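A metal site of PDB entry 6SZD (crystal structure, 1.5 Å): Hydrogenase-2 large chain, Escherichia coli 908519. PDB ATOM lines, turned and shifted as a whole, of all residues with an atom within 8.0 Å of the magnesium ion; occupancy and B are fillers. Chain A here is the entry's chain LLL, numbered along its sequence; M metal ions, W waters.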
ATOM      1  N   TRP A  38      -9.613  -5.609  -0.828  1.00  0.00           N
ATOM      2  CA  TRP A  38      -8.256  -6.145  -0.574  1.00  0.00           C
ATOM      3  C   TRP A  38      -7.227  -5.355  -1.352  1.00  0.00           C
ATOM      4  O   TRP A  38      -7.516  -4.871  -2.435  1.00  0.00           O
ATOM      5  CB  TRP A  38      -8.191  -7.629  -0.926  1.00  0.00           C
ATOM      6  CG  TRP A  38      -6.882  -8.326  -0.770  1.00  0.00           C
ATOM      7  CD1 TRP A  38      -6.243  -8.705   0.379  1.00  0.00           C
ATOM      8  CD2 TRP A  38      -6.079  -8.843  -1.839  1.00  0.00           C
ATOM      9  NE1 TRP A  38      -5.067  -9.348   0.091  1.00  0.00           N
ATOM     10  CE2 TRP A  38      -4.953  -9.454  -1.268  1.00  0.00           C
ATOM     11  CE3 TRP A  38      -6.180  -8.792  -3.232  1.00  0.00           C
ATOM     12  CZ2 TRP A  38      -3.967 -10.059  -2.051  1.00  0.00           C
ATOM     13  CZ3 TRP A  38      -5.188  -9.365  -4.012  1.00  0.00           C
ATOM     14  CH2 TRP A  38      -4.099 -10.004  -3.419  1.00  0.00           C
ATOM     15  N   GLU A  42       0.604  -7.536   2.222  1.00  0.00           N
ATOM     16  CA  GLU A  42       1.628  -8.579   2.525  1.00  0.00           C
ATOM     17  C   GLU A  42       2.492  -8.874   1.307  1.00  0.00           C
ATOM     18  O   GLU A  42       3.703  -9.032   1.468  1.00  0.00           O
ATOM     19  CB  GLU A  42       0.967  -9.844   3.031  1.00  0.00           C
ATOM     20  CG  GLU A  42       0.331  -9.659   4.389  1.00  0.00           C
ATOM     21  CD  GLU A  42      -0.787 -10.632   4.733  1.00  0.00           C
ATOM     22  OE1 GLU A  42      -1.482 -11.088   3.817  1.00  0.00           O
ATOM     23  OE2 GLU A  42      -0.981 -10.874   5.950  1.00  0.00           O
ATOM     24  N   ILE A  60      -1.206  -0.146   6.157  1.00  0.00           N
ATOM     25  CA  ILE A  60      -2.368  -1.050   6.326  1.00  0.00           C
ATOM     26  C   ILE A  60      -3.541  -0.224   6.830  1.00  0.00           C
ATOM     27  O   ILE A  60      -4.699  -0.474   6.347  1.00  0.00           O
ATOM     28  CB  ILE A  60      -2.029  -2.247   7.211  1.00  0.00           C
ATOM     29  CG1 ILE A  60      -1.146  -3.228   6.453  1.00  0.00           C
ATOM     30  CG2 ILE A  60      -3.292  -2.904   7.729  1.00  0.00           C
ATOM     31  CD1 ILE A  60      -0.576  -4.326   7.304  1.00  0.00           C
ATOM     32  N   GLU A 329      -4.218 -19.274  10.662  1.00  0.00           N
ATOM     33  CA  GLU A 329      -5.313 -18.678   9.877  1.00  0.00           C
ATOM     34  C   GLU A 329      -5.733 -19.634   8.768  1.00  0.00           C
ATOM     35  O   GLU A 329      -4.846 -20.281   8.156  1.00  0.00           O
ATOM     36  CB  GLU A 329      -4.897 -17.361   9.220  1.00  0.00           C
ATOM     37  CG  GLU A 329      -4.542 -16.286  10.231  1.00  0.00           C
ATOM     38  CD  GLU A 329      -4.046 -15.046   9.508  1.00  0.00           C
ATOM     39  OE1 GLU A 329      -2.946 -15.151   8.887  1.00  0.00           O
ATOM     40  OE2 GLU A 329      -4.770 -13.991   9.526  1.00  0.00           O
ATOM     41  N   TYR A 336      -9.201 -16.788  -0.754  1.00  0.00           N
ATOM     42  CA  TYR A 336      -7.804 -17.184  -0.998  1.00  0.00           C
ATOM     43  C   TYR A 336      -7.808 -18.685  -1.352  1.00  0.00           C
ATOM     44  O   TYR A 336      -8.771 -19.437  -0.976  1.00  0.00           O
ATOM     45  CB  TYR A 336      -6.881 -16.856   0.172  1.00  0.00           C
ATOM     46  CG  TYR A 336      -6.975 -15.406   0.621  1.00  0.00           C
ATOM     47  CD1 TYR A 336      -6.395 -14.362  -0.096  1.00  0.00           C
ATOM     48  CD2 TYR A 336      -7.719 -15.099   1.731  1.00  0.00           C
ATOM     49  CE1 TYR A 336      -6.547 -13.052   0.302  1.00  0.00           C
ATOM     50  CE2 TYR A 336      -7.864 -13.789   2.154  1.00  0.00           C
ATOM     51  CZ  TYR A 336      -7.273 -12.773   1.438  1.00  0.00           C
ATOM     52  OH  TYR A 336      -7.448 -11.461   1.856  1.00  0.00           O
ATOM     53  N   PRO A 344       1.511 -18.384  10.500  1.00  0.00           N
ATOM     54  CA  PRO A 344       1.793 -17.228   9.653  1.00  0.00           C
ATOM     55  C   PRO A 344       3.197 -17.186   9.034  1.00  0.00           C
ATOM     56  O   PRO A 344       3.339 -16.632   7.962  1.00  0.00           O
ATOM     57  CB  PRO A 344       1.562 -16.035  10.594  1.00  0.00           C
ATOM     58  CG  PRO A 344       0.560 -16.572  11.590  1.00  0.00           C
ATOM     59  CD  PRO A 344       1.028 -17.999  11.823  1.00  0.00           C
ATOM     60  N   THR A 348       0.309 -18.122   3.203  1.00  0.00           N
ATOM     61  CA  THR A 348       0.158 -17.599   1.821  1.00  0.00           C
ATOM     62  C   THR A 348      -1.075 -16.694   1.760  1.00  0.00           C
ATOM     63  O   THR A 348      -1.901 -16.775   2.619  1.00  0.00           O
ATOM     64  CB  THR A 348       0.092 -18.724   0.776  1.00  0.00           C
ATOM     65  OG1 THR A 348      -1.129 -19.418   1.000  1.00  0.00           O
ATOM     66  CG2 THR A 348       1.310 -19.629   0.819  1.00  0.00           C
ATOM     67  N   THR A 349      -1.107 -15.821   0.760  1.00  0.00           N
ATOM     68  CA  THR A 349      -2.230 -14.906   0.514  1.00  0.00           C
ATOM     69  C   THR A 349      -2.478 -14.885  -0.975  1.00  0.00           C
ATOM     70  O   THR A 349      -2.132 -13.890  -1.638  1.00  0.00           O
ATOM     71  CB  THR A 349      -1.936 -13.535   1.119  1.00  0.00           C
ATOM     72  OG1 THR A 349      -1.483 -13.746   2.459  1.00  0.00           O
ATOM     73  CG2 THR A 349      -3.169 -12.659   1.110  1.00  0.00           C
ATOM     74  N   TRP A 364     -12.852 -11.277   2.179  1.00  0.00           N
ATOM     75  CA  TRP A 364     -11.384 -11.118   2.053  1.00  0.00           C
ATOM     76  C   TRP A 364     -10.684 -11.275   3.403  1.00  0.00           C
ATOM     77  O   TRP A 364      -9.447 -11.270   3.428  1.00  0.00           O
ATOM     78  CB  TRP A 364     -11.026  -9.791   1.403  1.00  0.00           C
ATOM     79  CG  TRP A 364     -11.325  -9.725  -0.060  1.00  0.00           C
ATOM     80  CD1 TRP A 364     -12.316  -9.042  -0.667  1.00  0.00           C
ATOM     81  CD2 TRP A 364     -10.628 -10.429  -1.089  1.00  0.00           C
ATOM     82  NE1 TRP A 364     -12.289  -9.275  -2.019  1.00  0.00           N
ATOM     83  CE2 TRP A 364     -11.239 -10.082  -2.309  1.00  0.00           C
ATOM     84  CE3 TRP A 364      -9.495 -11.251  -1.084  1.00  0.00           C
ATOM     85  CZ2 TRP A 364     -10.795 -10.631  -3.514  1.00  0.00           C
ATOM     86  CZ3 TRP A 364      -9.048 -11.772  -2.273  1.00  0.00           C
ATOM     87  CH2 TRP A 364      -9.728 -11.489  -3.457  1.00  0.00           C
ATOM     88  N   VAL A 365     -11.409 -11.370   4.501  1.00  0.00           N
ATOM     89  CA  VAL A 365     -10.799 -11.596   5.829  1.00  0.00           C
ATOM     90  C   VAL A 365     -10.493 -13.087   5.983  1.00  0.00           C
ATOM     91  O   VAL A 365     -11.353 -13.920   5.669  1.00  0.00           O
ATOM     92  CB  VAL A 365     -11.716 -11.115   6.970  1.00  0.00           C
ATOM     93  CG1 VAL A 365     -10.970 -11.133   8.293  1.00  0.00           C
ATOM     94  CG2 VAL A 365     -12.277  -9.725   6.725  1.00  0.00           C
ATOM     95  N   LYS A 366      -9.319 -13.423   6.461  1.00  0.00           N
ATOM     96  CA  LYS A 366      -8.966 -14.801   6.880  1.00  0.00           C
ATOM     97  C   LYS A 366      -9.614 -15.128   8.218  1.00  0.00           C
ATOM     98  O   LYS A 366     -10.127 -14.215   8.900  1.00  0.00           O
ATOM     99  CB  LYS A 366      -7.446 -14.977   6.930  1.00  0.00           C
ATOM    100  CG  LYS A 366      -6.733 -14.890   5.611  1.00  0.00           C
ATOM    101  CD  LYS A 366      -5.238 -14.961   5.776  1.00  0.00           C
ATOM    102  CE  LYS A 366      -4.487 -14.997   4.474  1.00  0.00           C
ATOM    103  NZ  LYS A 366      -3.048 -15.065   4.697  1.00  0.00           N
ATOM    104  N   PRO A 368      -8.701 -16.532  11.788  1.00  0.00           N
ATOM    105  CA  PRO A 368      -7.674 -16.941  12.733  1.00  0.00           C
ATOM    106  C   PRO A 368      -8.222 -17.833  13.850  1.00  0.00           C
ATOM    107  O   PRO A 368      -9.352 -17.628  14.291  1.00  0.00           O
ATOM    108  CB  PRO A 368      -7.162 -15.633  13.361  1.00  0.00           C
ATOM    109  CG  PRO A 368      -7.704 -14.554  12.434  1.00  0.00           C
ATOM    110  CD  PRO A 368      -9.011 -15.092  11.940  1.00  0.00           C
ATOM    111  N   SER A 483      -0.203  -8.981  15.384  1.00  0.00           N
ATOM    112  CA  SER A 483       1.099  -9.624  15.173  1.00  0.00           C
ATOM    113  C   SER A 483       1.505  -9.483  13.706  1.00  0.00           C
ATOM    114  O   SER A 483       0.690  -9.716  12.815  1.00  0.00           O
ATOM    115  CB  SER A 483       1.142 -11.071  15.633  1.00  0.00           C
ATOM    116  OG  SER A 483       0.084 -11.840  15.113  1.00  0.00           O
ATOM    117  N   TRP A 485       4.522 -11.022  11.134  1.00  0.00           N
ATOM    118  CA  TRP A 485       5.362 -12.230  11.028  1.00  0.00           C
ATOM    119  C   TRP A 485       6.252 -12.096   9.792  1.00  0.00           C
ATOM    120  O   TRP A 485       5.744 -12.047   8.680  1.00  0.00           O
ATOM    121  CB  TRP A 485       4.484 -13.479  10.944  1.00  0.00           C
ATOM    122  CG  TRP A 485       3.521 -13.636  12.077  1.00  0.00           C
ATOM    123  CD1 TRP A 485       2.384 -12.914  12.289  1.00  0.00           C
ATOM    124  CD2 TRP A 485       3.571 -14.622  13.116  1.00  0.00           C
ATOM    125  NE1 TRP A 485       1.735 -13.384  13.394  1.00  0.00           N
ATOM    126  CE2 TRP A 485       2.431 -14.439  13.915  1.00  0.00           C
ATOM    127  CE3 TRP A 485       4.480 -15.645  13.433  1.00  0.00           C
ATOM    128  CZ2 TRP A 485       2.192 -15.224  15.046  1.00  0.00           C
ATOM    129  CZ3 TRP A 485       4.210 -16.433  14.542  1.00  0.00           C
ATOM    130  CH2 TRP A 485       3.074 -16.229  15.311  1.00  0.00           C
ATOM    131  N   TYR A 496       5.865 -12.331   4.533  1.00  0.00           N
ATOM    132  CA  TYR A 496       5.353 -11.305   5.471  1.00  0.00           C
ATOM    133  C   TYR A 496       3.870 -11.595   5.662  1.00  0.00           C
ATOM    134  O   TYR A 496       3.128 -11.660   4.660  1.00  0.00           O
ATOM    135  CB  TYR A 496       5.564  -9.888   4.960  1.00  0.00           C
ATOM    136  CG  TYR A 496       5.584  -8.872   6.078  1.00  0.00           C
ATOM    137  CD1 TYR A 496       4.407  -8.373   6.608  1.00  0.00           C
ATOM    138  CD2 TYR A 496       6.785  -8.414   6.597  1.00  0.00           C
ATOM    139  CE1 TYR A 496       4.411  -7.475   7.660  1.00  0.00           C
ATOM    140  CE2 TYR A 496       6.795  -7.504   7.638  1.00  0.00           C
ATOM    141  CZ  TYR A 496       5.609  -7.008   8.158  1.00  0.00           C
ATOM    142  OH  TYR A 496       5.698  -6.115   9.187  1.00  0.00           O
ATOM    143  N   GLN A 497       3.448 -11.807   6.896  1.00  0.00           N
ATOM    144  CA  GLN A 497       2.024 -12.084   7.207  1.00  0.00           C
ATOM    145  C   GLN A 497       1.630 -11.195   8.390  1.00  0.00           C
ATOM    146  O   GLN A 497       2.329 -11.260   9.422  1.00  0.00           O
ATOM    147  CB  GLN A 497       1.801 -13.568   7.472  1.00  0.00           C
ATOM    148  CG  GLN A 497       1.963 -14.447   6.241  1.00  0.00           C
ATOM    149  CD  GLN A 497       0.887 -14.276   5.190  1.00  0.00           C
ATOM    150  OE1 GLN A 497      -0.297 -14.084   5.536  1.00  0.00           O
ATOM    151  NE2 GLN A 497       1.251 -14.380   3.916  1.00  0.00           N
ATOM    152  N   ALA A 498       0.554 -10.443   8.227  1.00  0.00           N
ATOM    153  CA  ALA A 498      -0.079  -9.693   9.310  1.00  0.00           C
ATOM    154  C   ALA A 498      -1.342 -10.410   9.774  1.00  0.00           C
ATOM    155  O   ALA A 498      -2.170 -10.771   8.934  1.00  0.00           O
ATOM    156  CB  ALA A 498      -0.391  -8.292   8.876  1.00  0.00           C
ATOM    157  N   VAL A 499      -1.447 -10.630  11.081  1.00  0.00           N
ATOM    158  CA  VAL A 499      -2.651 -11.201  11.738  1.00  0.00           C
ATOM    159  C   VAL A 499      -3.167 -10.083  12.642  1.00  0.00           C
ATOM    160  O   VAL A 499      -2.495  -9.756  13.629  1.00  0.00           O
ATOM    161  CB  VAL A 499      -2.396 -12.503  12.503  1.00  0.00           C
ATOM    162  CG1 VAL A 499      -3.689 -13.133  12.949  1.00  0.00           C
ATOM    163  CG2 VAL A 499      -1.570 -13.481  11.676  1.00  0.00           C
ATOM    164  N   VAL A 500      -4.266  -9.471  12.263  1.00  0.00           N
ATOM    165  CA  VAL A 500      -4.639  -8.137  12.784  1.00  0.00           C
ATOM    166  C   VAL A 500      -5.853  -8.321  13.675  1.00  0.00           C
ATOM    167  O   VAL A 500      -6.612  -9.257  13.501  1.00  0.00           O
ATOM    168  CB  VAL A 500      -4.845  -7.174  11.604  1.00  0.00           C
ATOM    169  CG1 VAL A 500      -5.067  -5.741  12.024  1.00  0.00           C
ATOM    170  CG2 VAL A 500      -3.633  -7.247  10.670  1.00  0.00           C
ATOM    171  N   THR A 503      -9.045  -8.972  12.099  1.00  0.00           N
ATOM    172  CA  THR A 503      -9.035 -10.310  11.434  1.00  0.00           C
ATOM    173  C   THR A 503      -9.644 -11.327  12.430  1.00  0.00           C
ATOM    174  O   THR A 503     -10.509 -12.118  12.007  1.00  0.00           O
ATOM    175  CB  THR A 503      -7.635 -10.751  10.962  1.00  0.00           C
ATOM    176  OG1 THR A 503      -6.947  -9.654  10.355  1.00  0.00           O
ATOM    177  CG2 THR A 503      -7.770 -11.904   9.979  1.00  0.00           C
ATOM    178  N   CYS A 549      -7.453  -2.895   8.193  1.00  0.00           N
ATOM    179  CA  CYS A 549      -6.733  -3.779   9.133  1.00  0.00           C
ATOM    180  C   CYS A 549      -7.102  -5.241   8.930  1.00  0.00           C
ATOM    181  O   CYS A 549      -6.207  -6.095   8.821  1.00  0.00           O
ATOM    182  CB  CYS A 549      -7.030  -3.424  10.580  1.00  0.00           C
ATOM    183  SG  CYS A 549      -5.939  -2.120  11.189  1.00  0.00           S
ATOM    184  N   ALA A 550      -8.394  -5.575   8.868  1.00  0.00           N
ATOM    185  CA  ALA A 550      -8.793  -6.998   8.909  1.00  0.00           C
ATOM    186  C   ALA A 550      -8.229  -7.720   7.670  1.00  0.00           C
ATOM    187  O   ALA A 550      -7.829  -8.857   7.807  1.00  0.00           O
ATOM    188  CB  ALA A 550     -10.285  -7.105   8.918  1.00  0.00           C
ATOM    189  N   VAL A 551      -8.226  -7.017   6.532  1.00  0.00           N
ATOM    190  CA  VAL A 551      -7.929  -7.620   5.202  1.00  0.00           C
ATOM    191  C   VAL A 551      -6.499  -7.300   4.733  1.00  0.00           C
ATOM    192  O   VAL A 551      -5.847  -8.212   4.175  1.00  0.00           O
ATOM    193  CB  VAL A 551      -8.930  -7.151   4.152  1.00  0.00           C
ATOM    194  CG1 VAL A 551      -8.531  -7.683   2.794  1.00  0.00           C
ATOM    195  CG2 VAL A 551     -10.333  -7.555   4.476  1.00  0.00           C
ATOM    196  N   HIS A 552      -6.069  -6.051   4.821  1.00  0.00           N
ATOM    197  CA  HIS A 552      -4.721  -5.597   4.360  1.00  0.00           C
ATOM    198  C   HIS A 552      -4.493  -6.059   2.907  1.00  0.00           C
ATOM    199  O   HIS A 552      -3.385  -6.629   2.620  1.00  0.00           O
ATOM    200  CB  HIS A 552      -3.617  -5.960   5.376  1.00  0.00           C
ATOM    201  CG  HIS A 552      -3.714  -7.288   6.045  1.00  0.00           C
ATOM    202  ND1 HIS A 552      -4.567  -7.503   7.116  1.00  0.00           N
ATOM    203  CD2 HIS A 552      -3.082  -8.447   5.787  1.00  0.00           C
ATOM    204  CE1 HIS A 552      -4.423  -8.782   7.500  1.00  0.00           C
ATOM    205  NE2 HIS A 552      -3.523  -9.375   6.690  1.00  0.00           N
HETATM  206 MG    MG M   1      -2.842 -11.385   7.001  1.00  0.00          MG
HETATM  207  O   HOH W   1      -2.013 -13.287   7.287  1.00  0.00           O
HETATM  208  O   HOH W   2      -3.531 -12.001   5.063  1.00  0.00           O
HETATM  209  O   HOH W   3      -4.653 -11.957   7.946  1.00  0.00           O
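The backbone carbonyl oxygen (O) of Cys 549 sits at hydrogen-bond distance from a ring nitrogen (ND1) of His 552 (2.8 Å).
The side-chain carboxylate of Glu 42 lies close to the side-chain amide oxygen of Gln 497, at 3.3 Å.
OE1 of Glu 42 lies within hydrogen-bond range of OG1 of Thr 349.
OE1 of Gln 497 lies within hydrogen-bond range of NZ of Lys 366 (3.0 Å).
OG1 of Thr 349 lies within hydrogen-bond range of NE2 of Gln 497.
The backbone carbonyl oxygen of Gln 497 is in hydrogen-bond range of the backbone NH of Trp 485, 2.8 Å away.
Merely in contact with the magnesium ion: Gln 497.
Four residues have an atom within 4 Å of the magnesium ion: Glu 42, Gln 497, Ala 498 and His 552.
Water W1 is bound to the magnesium ion, 2.1 Å away.
Water W3 is bound to the magnesium ion, 2.1 Å away.
O of Ala 498 binds the magnesium ion (2.1 Å).
NE2 of His 552 is bound to the magnesium ion (2.1 Å).
Water W2 is bound to the magnesium ion (2.1 Å).
OE2 of Glu 42 binds the magnesium ion (2.2 Å).
The magnesium ion has six donor atoms within binding distance.
Water W1 lies within hydrogen-bond range of the side-chain amide oxygen (OE1) of Gln 497, the side-chain carboxylate (OE1) of Glu 329 and the side-chain amino group (NZ) of Lys 366.
Water W2 bridges the side-chain carboxylate of Glu 42 and the side-chain amino group of Lys 366.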
